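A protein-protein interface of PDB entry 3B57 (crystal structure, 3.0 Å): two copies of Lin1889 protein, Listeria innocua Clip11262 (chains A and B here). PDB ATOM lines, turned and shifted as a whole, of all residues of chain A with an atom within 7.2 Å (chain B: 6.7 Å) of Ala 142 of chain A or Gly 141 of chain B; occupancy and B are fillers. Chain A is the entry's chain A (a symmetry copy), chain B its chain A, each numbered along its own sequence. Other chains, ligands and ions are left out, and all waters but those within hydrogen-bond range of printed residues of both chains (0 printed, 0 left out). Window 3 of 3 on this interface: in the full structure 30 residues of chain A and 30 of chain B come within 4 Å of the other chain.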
ATOM      1  N   THR A 136       8.057  25.188 -18.320  1.00  0.00           N
ATOM      2  CA  THR A 136       6.937  26.038 -17.942  1.00  0.00           C
ATOM      3  C   THR A 136       5.573  25.441 -18.299  1.00  0.00           C
ATOM      4  O   THR A 136       4.606  25.615 -17.559  1.00  0.00           O
ATOM      5  CB  THR A 136       7.073  27.451 -18.546  1.00  0.00           C
ATOM      6  OG1 THR A 136       5.957  28.248 -18.136  1.00  0.00           O
ATOM      7  CG2 THR A 136       7.122  27.397 -20.051  1.00  0.00           C
ATOM      8  N   PHE A 137       5.488  24.730 -19.420  1.00  0.00           N
ATOM      9  CA  PHE A 137       4.227  24.103 -19.785  1.00  0.00           C
ATOM     10  C   PHE A 137       3.986  22.867 -18.931  1.00  0.00           C
ATOM     11  O   PHE A 137       2.833  22.519 -18.684  1.00  0.00           O
ATOM     12  CB  PHE A 137       4.188  23.737 -21.268  1.00  0.00           C
ATOM     13  CG  PHE A 137       3.759  24.863 -22.138  1.00  0.00           C
ATOM     14  CD1 PHE A 137       2.490  25.419 -21.980  1.00  0.00           C
ATOM     15  CD2 PHE A 137       4.649  25.433 -23.052  1.00  0.00           C
ATOM     16  CE1 PHE A 137       2.112  26.540 -22.711  1.00  0.00           C
ATOM     17  CE2 PHE A 137       4.297  26.560 -23.801  1.00  0.00           C
ATOM     18  CZ  PHE A 137       3.023  27.120 -23.632  1.00  0.00           C
ATOM     19  N   THR A 138       5.047  22.194 -18.479  1.00  0.00           N
ATOM     20  CA  THR A 138       4.837  21.022 -17.626  1.00  0.00           C
ATOM     21  C   THR A 138       4.377  21.504 -16.269  1.00  0.00           C
ATOM     22  O   THR A 138       3.598  20.840 -15.593  1.00  0.00           O
ATOM     23  CB  THR A 138       6.096  20.186 -17.369  1.00  0.00           C
ATOM     24  OG1 THR A 138       6.596  19.642 -18.598  1.00  0.00           O
ATOM     25  CG2 THR A 138       5.744  19.034 -16.423  1.00  0.00           C
ATOM     26  N   TYR A 139       4.874  22.671 -15.876  1.00  0.00           N
ATOM     27  CA  TYR A 139       4.509  23.254 -14.595  1.00  0.00           C
ATOM     28  C   TYR A 139       3.042  23.656 -14.624  1.00  0.00           C
ATOM     29  O   TYR A 139       2.286  23.354 -13.698  1.00  0.00           O
ATOM     30  CB  TYR A 139       5.397  24.467 -14.299  1.00  0.00           C
ATOM     31  CG  TYR A 139       4.968  25.262 -13.094  1.00  0.00           C
ATOM     32  CD1 TYR A 139       4.059  26.318 -13.225  1.00  0.00           C
ATOM     33  CD2 TYR A 139       5.442  24.941 -11.817  1.00  0.00           C
ATOM     34  CE1 TYR A 139       3.629  27.036 -12.118  1.00  0.00           C
ATOM     35  CE2 TYR A 139       5.017  25.651 -10.699  1.00  0.00           C
ATOM     36  CZ  TYR A 139       4.108  26.698 -10.857  1.00  0.00           C
ATOM     37  OH  TYR A 139       3.677  27.402  -9.756  1.00  0.00           O
ATOM     38  N   GLY A 140       2.645  24.331 -15.701  1.00  0.00           N
ATOM     39  CA  GLY A 140       1.260  24.747 -15.841  1.00  0.00           C
ATOM     40  C   GLY A 140       0.329  23.547 -15.781  1.00  0.00           C
ATOM     41  O   GLY A 140      -0.793  23.639 -15.277  1.00  0.00           O
ATOM     42  N   GLY A 141       0.806  22.413 -16.288  1.00  0.00           N
ATOM     43  CA  GLY A 141       0.009  21.200 -16.292  1.00  0.00           C
ATOM     44  C   GLY A 141      -0.088  20.525 -14.936  1.00  0.00           C
ATOM     45  O   GLY A 141      -0.595  19.407 -14.815  1.00  0.00           O
ATOM     46  N   ALA A 142       0.409  21.193 -13.907  1.00  0.00           N
ATOM     47  CA  ALA A 142       0.349  20.636 -12.567  1.00  0.00           C
ATOM     48  C   ALA A 142      -0.217  21.682 -11.623  1.00  0.00           C
ATOM     49  O   ALA A 142      -0.183  21.516 -10.408  1.00  0.00           O
ATOM     50  CB  ALA A 142       1.733  20.202 -12.110  1.00  0.00           C
ATOM     51  N   HIS A 143      -0.732  22.768 -12.186  1.00  0.00           N
ATOM     52  CA  HIS A 143      -1.312  23.832 -11.374  1.00  0.00           C
ATOM     53  C   HIS A 143      -2.501  24.425 -12.107  1.00  0.00           C
ATOM     54  O   HIS A 143      -2.932  25.545 -11.816  1.00  0.00           O
ATOM     55  CB  HIS A 143      -0.289  24.938 -11.109  1.00  0.00           C
ATOM     56  CG  HIS A 143       0.931  24.480 -10.372  1.00  0.00           C
ATOM     57  ND1 HIS A 143       1.742  23.461 -10.829  1.00  0.00           N
ATOM     58  CD2 HIS A 143       1.512  24.941  -9.239  1.00  0.00           C
ATOM     59  CE1 HIS A 143       2.769  23.316 -10.010  1.00  0.00           C
ATOM     60  NE2 HIS A 143       2.654  24.203  -9.038  1.00  0.00           N
ATOM     61  N   ASN A 144      -3.020  23.656 -13.063  1.00  0.00           N
ATOM     62  CA  ASN A 144      -4.160  24.061 -13.880  1.00  0.00           C
ATOM     63  C   ASN A 144      -4.049  25.489 -14.372  1.00  0.00           C
ATOM     64  O   ASN A 144      -4.891  26.328 -14.060  1.00  0.00           O
ATOM     65  CB  ASN A 144      -5.463  23.892 -13.101  1.00  0.00           C
ATOM     66  CG  ASN A 144      -5.875  22.443 -12.973  1.00  0.00           C
ATOM     67  OD1 ASN A 144      -5.145  21.622 -12.412  1.00  0.00           O
ATOM     68  ND2 ASN A 144      -7.054  22.118 -13.493  1.00  0.00           N
ATOM     69  N   ARG A 145      -3.003  25.762 -15.143  1.00  0.00           N
ATOM     70  CA  ARG A 145      -2.799  27.095 -15.683  1.00  0.00           C
ATOM     71  C   ARG A 145      -3.106  27.066 -17.179  1.00  0.00           C
ATOM     72  O   ARG A 145      -2.304  26.586 -17.982  1.00  0.00           O
ATOM     73  CB  ARG A 145      -1.356  27.554 -15.436  1.00  0.00           C
ATOM     74  CG  ARG A 145      -1.101  29.028 -15.774  1.00  0.00           C
ATOM     75  CD  ARG A 145       0.314  29.487 -15.405  1.00  0.00           C
ATOM     76  NE  ARG A 145       1.346  28.723 -16.102  1.00  0.00           N
ATOM     77  CZ  ARG A 145       2.606  28.621 -15.690  1.00  0.00           C
ATOM     78  NH1 ARG A 145       3.482  27.905 -16.385  1.00  0.00           N
ATOM     79  NH2 ARG A 145       2.988  29.226 -14.572  1.00  0.00           N
ATOM     80  N   THR B 136       0.853  18.809 -25.293  1.00  0.00           N
ATOM     81  CA  THR B 136       1.498  17.586 -24.838  1.00  0.00           C
ATOM     82  C   THR B 136       2.347  17.778 -23.578  1.00  0.00           C
ATOM     83  O   THR B 136       2.406  16.890 -22.728  1.00  0.00           O
ATOM     84  CB  THR B 136       2.346  16.946 -25.957  1.00  0.00           C
ATOM     85  OG1 THR B 136       2.946  15.744 -25.464  1.00  0.00           O
ATOM     86  CG2 THR B 136       3.424  17.886 -26.427  1.00  0.00           C
ATOM     87  N   PHE B 137       2.995  18.932 -23.444  1.00  0.00           N
ATOM     88  CA  PHE B 137       3.781  19.184 -22.246  1.00  0.00           C
ATOM     89  C   PHE B 137       2.867  19.512 -21.075  1.00  0.00           C
ATOM     90  O   PHE B 137       3.226  19.237 -19.932  1.00  0.00           O
ATOM     91  CB  PHE B 137       4.789  20.313 -22.461  1.00  0.00           C
ATOM     92  CG  PHE B 137       6.063  19.850 -23.071  1.00  0.00           C
ATOM     93  CD1 PHE B 137       6.859  18.923 -22.401  1.00  0.00           C
ATOM     94  CD2 PHE B 137       6.427  20.266 -24.355  1.00  0.00           C
ATOM     95  CE1 PHE B 137       7.998  18.401 -23.003  1.00  0.00           C
ATOM     96  CE2 PHE B 137       7.567  19.759 -24.985  1.00  0.00           C
ATOM     97  CZ  PHE B 137       8.358  18.820 -24.310  1.00  0.00           C
ATOM     98  N   THR B 138       1.694  20.098 -21.333  1.00  0.00           N
ATOM     99  CA  THR B 138       0.784  20.390 -20.223  1.00  0.00           C
ATOM    100  C   THR B 138       0.195  19.083 -19.742  1.00  0.00           C
ATOM    101  O   THR B 138      -0.086  18.914 -18.559  1.00  0.00           O
ATOM    102  CB  THR B 138      -0.411  21.277 -20.593  1.00  0.00           C
ATOM    103  OG1 THR B 138       0.039  22.567 -21.028  1.00  0.00           O
ATOM    104  CG2 THR B 138      -1.302  21.451 -19.359  1.00  0.00           C
ATOM    105  N   TYR B 139       0.008  18.160 -20.677  1.00  0.00           N
ATOM    106  CA  TYR B 139      -0.544  16.855 -20.350  1.00  0.00           C
ATOM    107  C   TYR B 139       0.453  16.084 -19.498  1.00  0.00           C
ATOM    108  O   TYR B 139       0.093  15.508 -18.469  1.00  0.00           O
ATOM    109  CB  TYR B 139      -0.869  16.086 -21.634  1.00  0.00           C
ATOM    110  CG  TYR B 139      -1.257  14.649 -21.408  1.00  0.00           C
ATOM    111  CD1 TYR B 139      -0.284  13.643 -21.389  1.00  0.00           C
ATOM    112  CD2 TYR B 139      -2.591  14.293 -21.178  1.00  0.00           C
ATOM    113  CE1 TYR B 139      -0.624  12.319 -21.146  1.00  0.00           C
ATOM    114  CE2 TYR B 139      -2.945  12.971 -20.931  1.00  0.00           C
ATOM    115  CZ  TYR B 139      -1.954  11.988 -20.916  1.00  0.00           C
ATOM    116  OH  TYR B 139      -2.294  10.678 -20.666  1.00  0.00           O
ATOM    117  N   GLY B 140       1.711  16.087 -19.932  1.00  0.00           N
ATOM    118  CA  GLY B 140       2.750  15.398 -19.185  1.00  0.00           C
ATOM    119  C   GLY B 140       2.837  15.934 -17.765  1.00  0.00           C
ATOM    120  O   GLY B 140       3.134  15.194 -16.824  1.00  0.00           O
ATOM    121  N   GLY B 141       2.562  17.227 -17.612  1.00  0.00           N
ATOM    122  CA  GLY B 141       2.614  17.856 -16.305  1.00  0.00           C
ATOM    123  C   GLY B 141       1.430  17.524 -15.415  1.00  0.00           C
ATOM    124  O   GLY B 141       1.255  18.106 -14.342  1.00  0.00           O
ATOM    125  N   ALA B 142       0.600  16.594 -15.861  1.00  0.00           N
ATOM    126  CA  ALA B 142      -0.554  16.197 -15.073  1.00  0.00           C
ATOM    127  C   ALA B 142      -0.583  14.682 -14.973  1.00  0.00           C
ATOM    128  O   ALA B 142      -1.567  14.101 -14.524  1.00  0.00           O
ATOM    129  CB  ALA B 142      -1.834  16.711 -15.712  1.00  0.00           C
ATOM    130  N   HIS B 143       0.496  14.040 -15.401  1.00  0.00           N
ATOM    131  CA  HIS B 143       0.579  12.585 -15.340  1.00  0.00           C
ATOM    132  C   HIS B 143       2.007  12.180 -15.027  1.00  0.00           C
ATOM    133  O   HIS B 143       2.412  11.040 -15.273  1.00  0.00           O
ATOM    134  CB  HIS B 143       0.165  11.958 -16.673  1.00  0.00           C
ATOM    135  CG  HIS B 143      -1.239  12.271 -17.088  1.00  0.00           C
ATOM    136  ND1 HIS B 143      -1.705  13.562 -17.236  1.00  0.00           N
ATOM    137  CD2 HIS B 143      -2.265  11.460 -17.442  1.00  0.00           C
ATOM    138  CE1 HIS B 143      -2.954  13.532 -17.665  1.00  0.00           C
ATOM    139  NE2 HIS B 143      -3.317  12.269 -17.800  1.00  0.00           N
ATOM    140  N   ASN B 144       2.761  13.134 -14.483  1.00  0.00           N
ATOM    141  CA  ASN B 144       4.162  12.934 -14.122  1.00  0.00           C
ATOM    142  C   ASN B 144       4.944  12.208 -15.197  1.00  0.00           C
ATOM    143  O   ASN B 144       5.475  11.125 -14.964  1.00  0.00           O
ATOM    144  CB  ASN B 144       4.269  12.163 -12.808  1.00  0.00           C
ATOM    145  CG  ASN B 144       3.924  13.017 -11.609  1.00  0.00           C
ATOM    146  OD1 ASN B 144       2.811  13.537 -11.499  1.00  0.00           O
ATOM    147  ND2 ASN B 144       4.880  13.167 -10.698  1.00  0.00           N
ATOM    148  N   ARG B 145       5.012  12.811 -16.378  1.00  0.00           N
ATOM    149  CA  ARG B 145       5.747  12.215 -17.481  1.00  0.00           C
ATOM    150  C   ARG B 145       7.031  13.012 -17.698  1.00  0.00           C
ATOM    151  O   ARG B 145       7.011  14.107 -18.264  1.00  0.00           O
ATOM    152  CB  ARG B 145       4.888  12.216 -18.752  1.00  0.00           C
ATOM    153  CG  ARG B 145       5.489  11.414 -19.914  1.00  0.00           C
ATOM    154  CD  ARG B 145       4.556  11.334 -21.128  1.00  0.00           C
ATOM    155  NE  ARG B 145       4.229  12.653 -21.666  1.00  0.00           N
ATOM    156  CZ  ARG B 145       3.164  12.907 -22.420  1.00  0.00           C
ATOM    157  NH1 ARG B 145       2.942  14.137 -22.869  1.00  0.00           N
ATOM    158  NH2 ARG B 145       2.312  11.934 -22.715  1.00  0.00           N
ATOM    159  N   THR B 157       8.206  12.395 -22.471  1.00  0.00           N
ATOM    160  CA  THR B 157       7.385  13.216 -23.349  1.00  0.00           C
ATOM    161  C   THR B 157       8.140  13.431 -24.670  1.00  0.00           C
ATOM    162  O   THR B 157       7.551  13.353 -25.751  1.00  0.00           O
ATOM    163  CB  THR B 157       7.068  14.581 -22.679  1.00  0.00           C
ATOM    164  OG1 THR B 157       6.335  14.354 -21.469  1.00  0.00           O
ATOM    165  CG2 THR B 157       6.239  15.474 -23.598  1.00  0.00           C
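Phe 137 of chain B touches its own counterpart, Phe 137 of chain A.
Phe 137 of chain A touches Thr 138 of chain B, and with the chains exchanged Thr 138 of chain A touches Phe 137 of chain B.
Thr 138 of chain A touches Gly 141 of chain B, and with the chains exchanged Gly 141 of chain A touches Thr 138 of chain B.
Gly 141 of chain A touches Ala 142 of chain B, and with the chains exchanged Ala 142 of chain A touches Gly 141 of chain B.
Of the 8 pairs that touch across the chains among the printed residues, 8 have their exchanged pair printed and touching as well.
Printed residues of chain A that touch a printed residue of chain B: Phe 137, Thr 138, Gly 141 and Ala 142.
Hydrophobic or aromatic side chains of chain A that line the printed part of chain B: Phe 137 and Ala 142.
Hydrophobic or aromatic side chains of chain B that line the printed part of chain A: Phe 137 and Ala 142.
Along chain B the printed residues that touch a printed residue of chain A span positions 137 to 142.
Of the printed residues of chain B, Phe 137 of chain A touches Phe 137 and Thr 138.
Of chain B, only Gly 141 (3.1 Å) comes within 4 Å of Ala 142 of chain A.
Of the printed residues of chain A, Phe 137 of chain B touches Phe 137 and Thr 138.
Printed residues of chain A within 4 Å of Thr 138 of chain B: Phe 137 and Gly 141.
No residue of chain A comes within 4 Å of Gly 140 of chain B.
Among the printed residues, merely in contact across the chains: Gly 141 of chain A with Thr 138 of chain B (3.2 Å), Thr 138 of chain A with Gly 141 of chain B (3.2 Å), Thr 138 of chain A with Phe 137 of chain B (3.3 Å), Phe 137 of chain A with Thr 138 of chain B (3.3 Å) and Phe 137 of chain A with Phe 137 of chain B (3.5 Å).
The backbone NH of Ala 142 of chain B lies close to the backbone carbonyl oxygen of Gly 141 of chain A, 3.2 Å away.
The backbone carbonyl oxygen of Gly 141 of chain B sits close to the backbone NH of Ala 142 of chain A, 3.2 Å away.
The backbone carbonyl oxygen (O) of Gly 141 of chain A lies close to the backbone carbonyl oxygen (O) of Gly 141 of chain B, 2.3 Å away.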
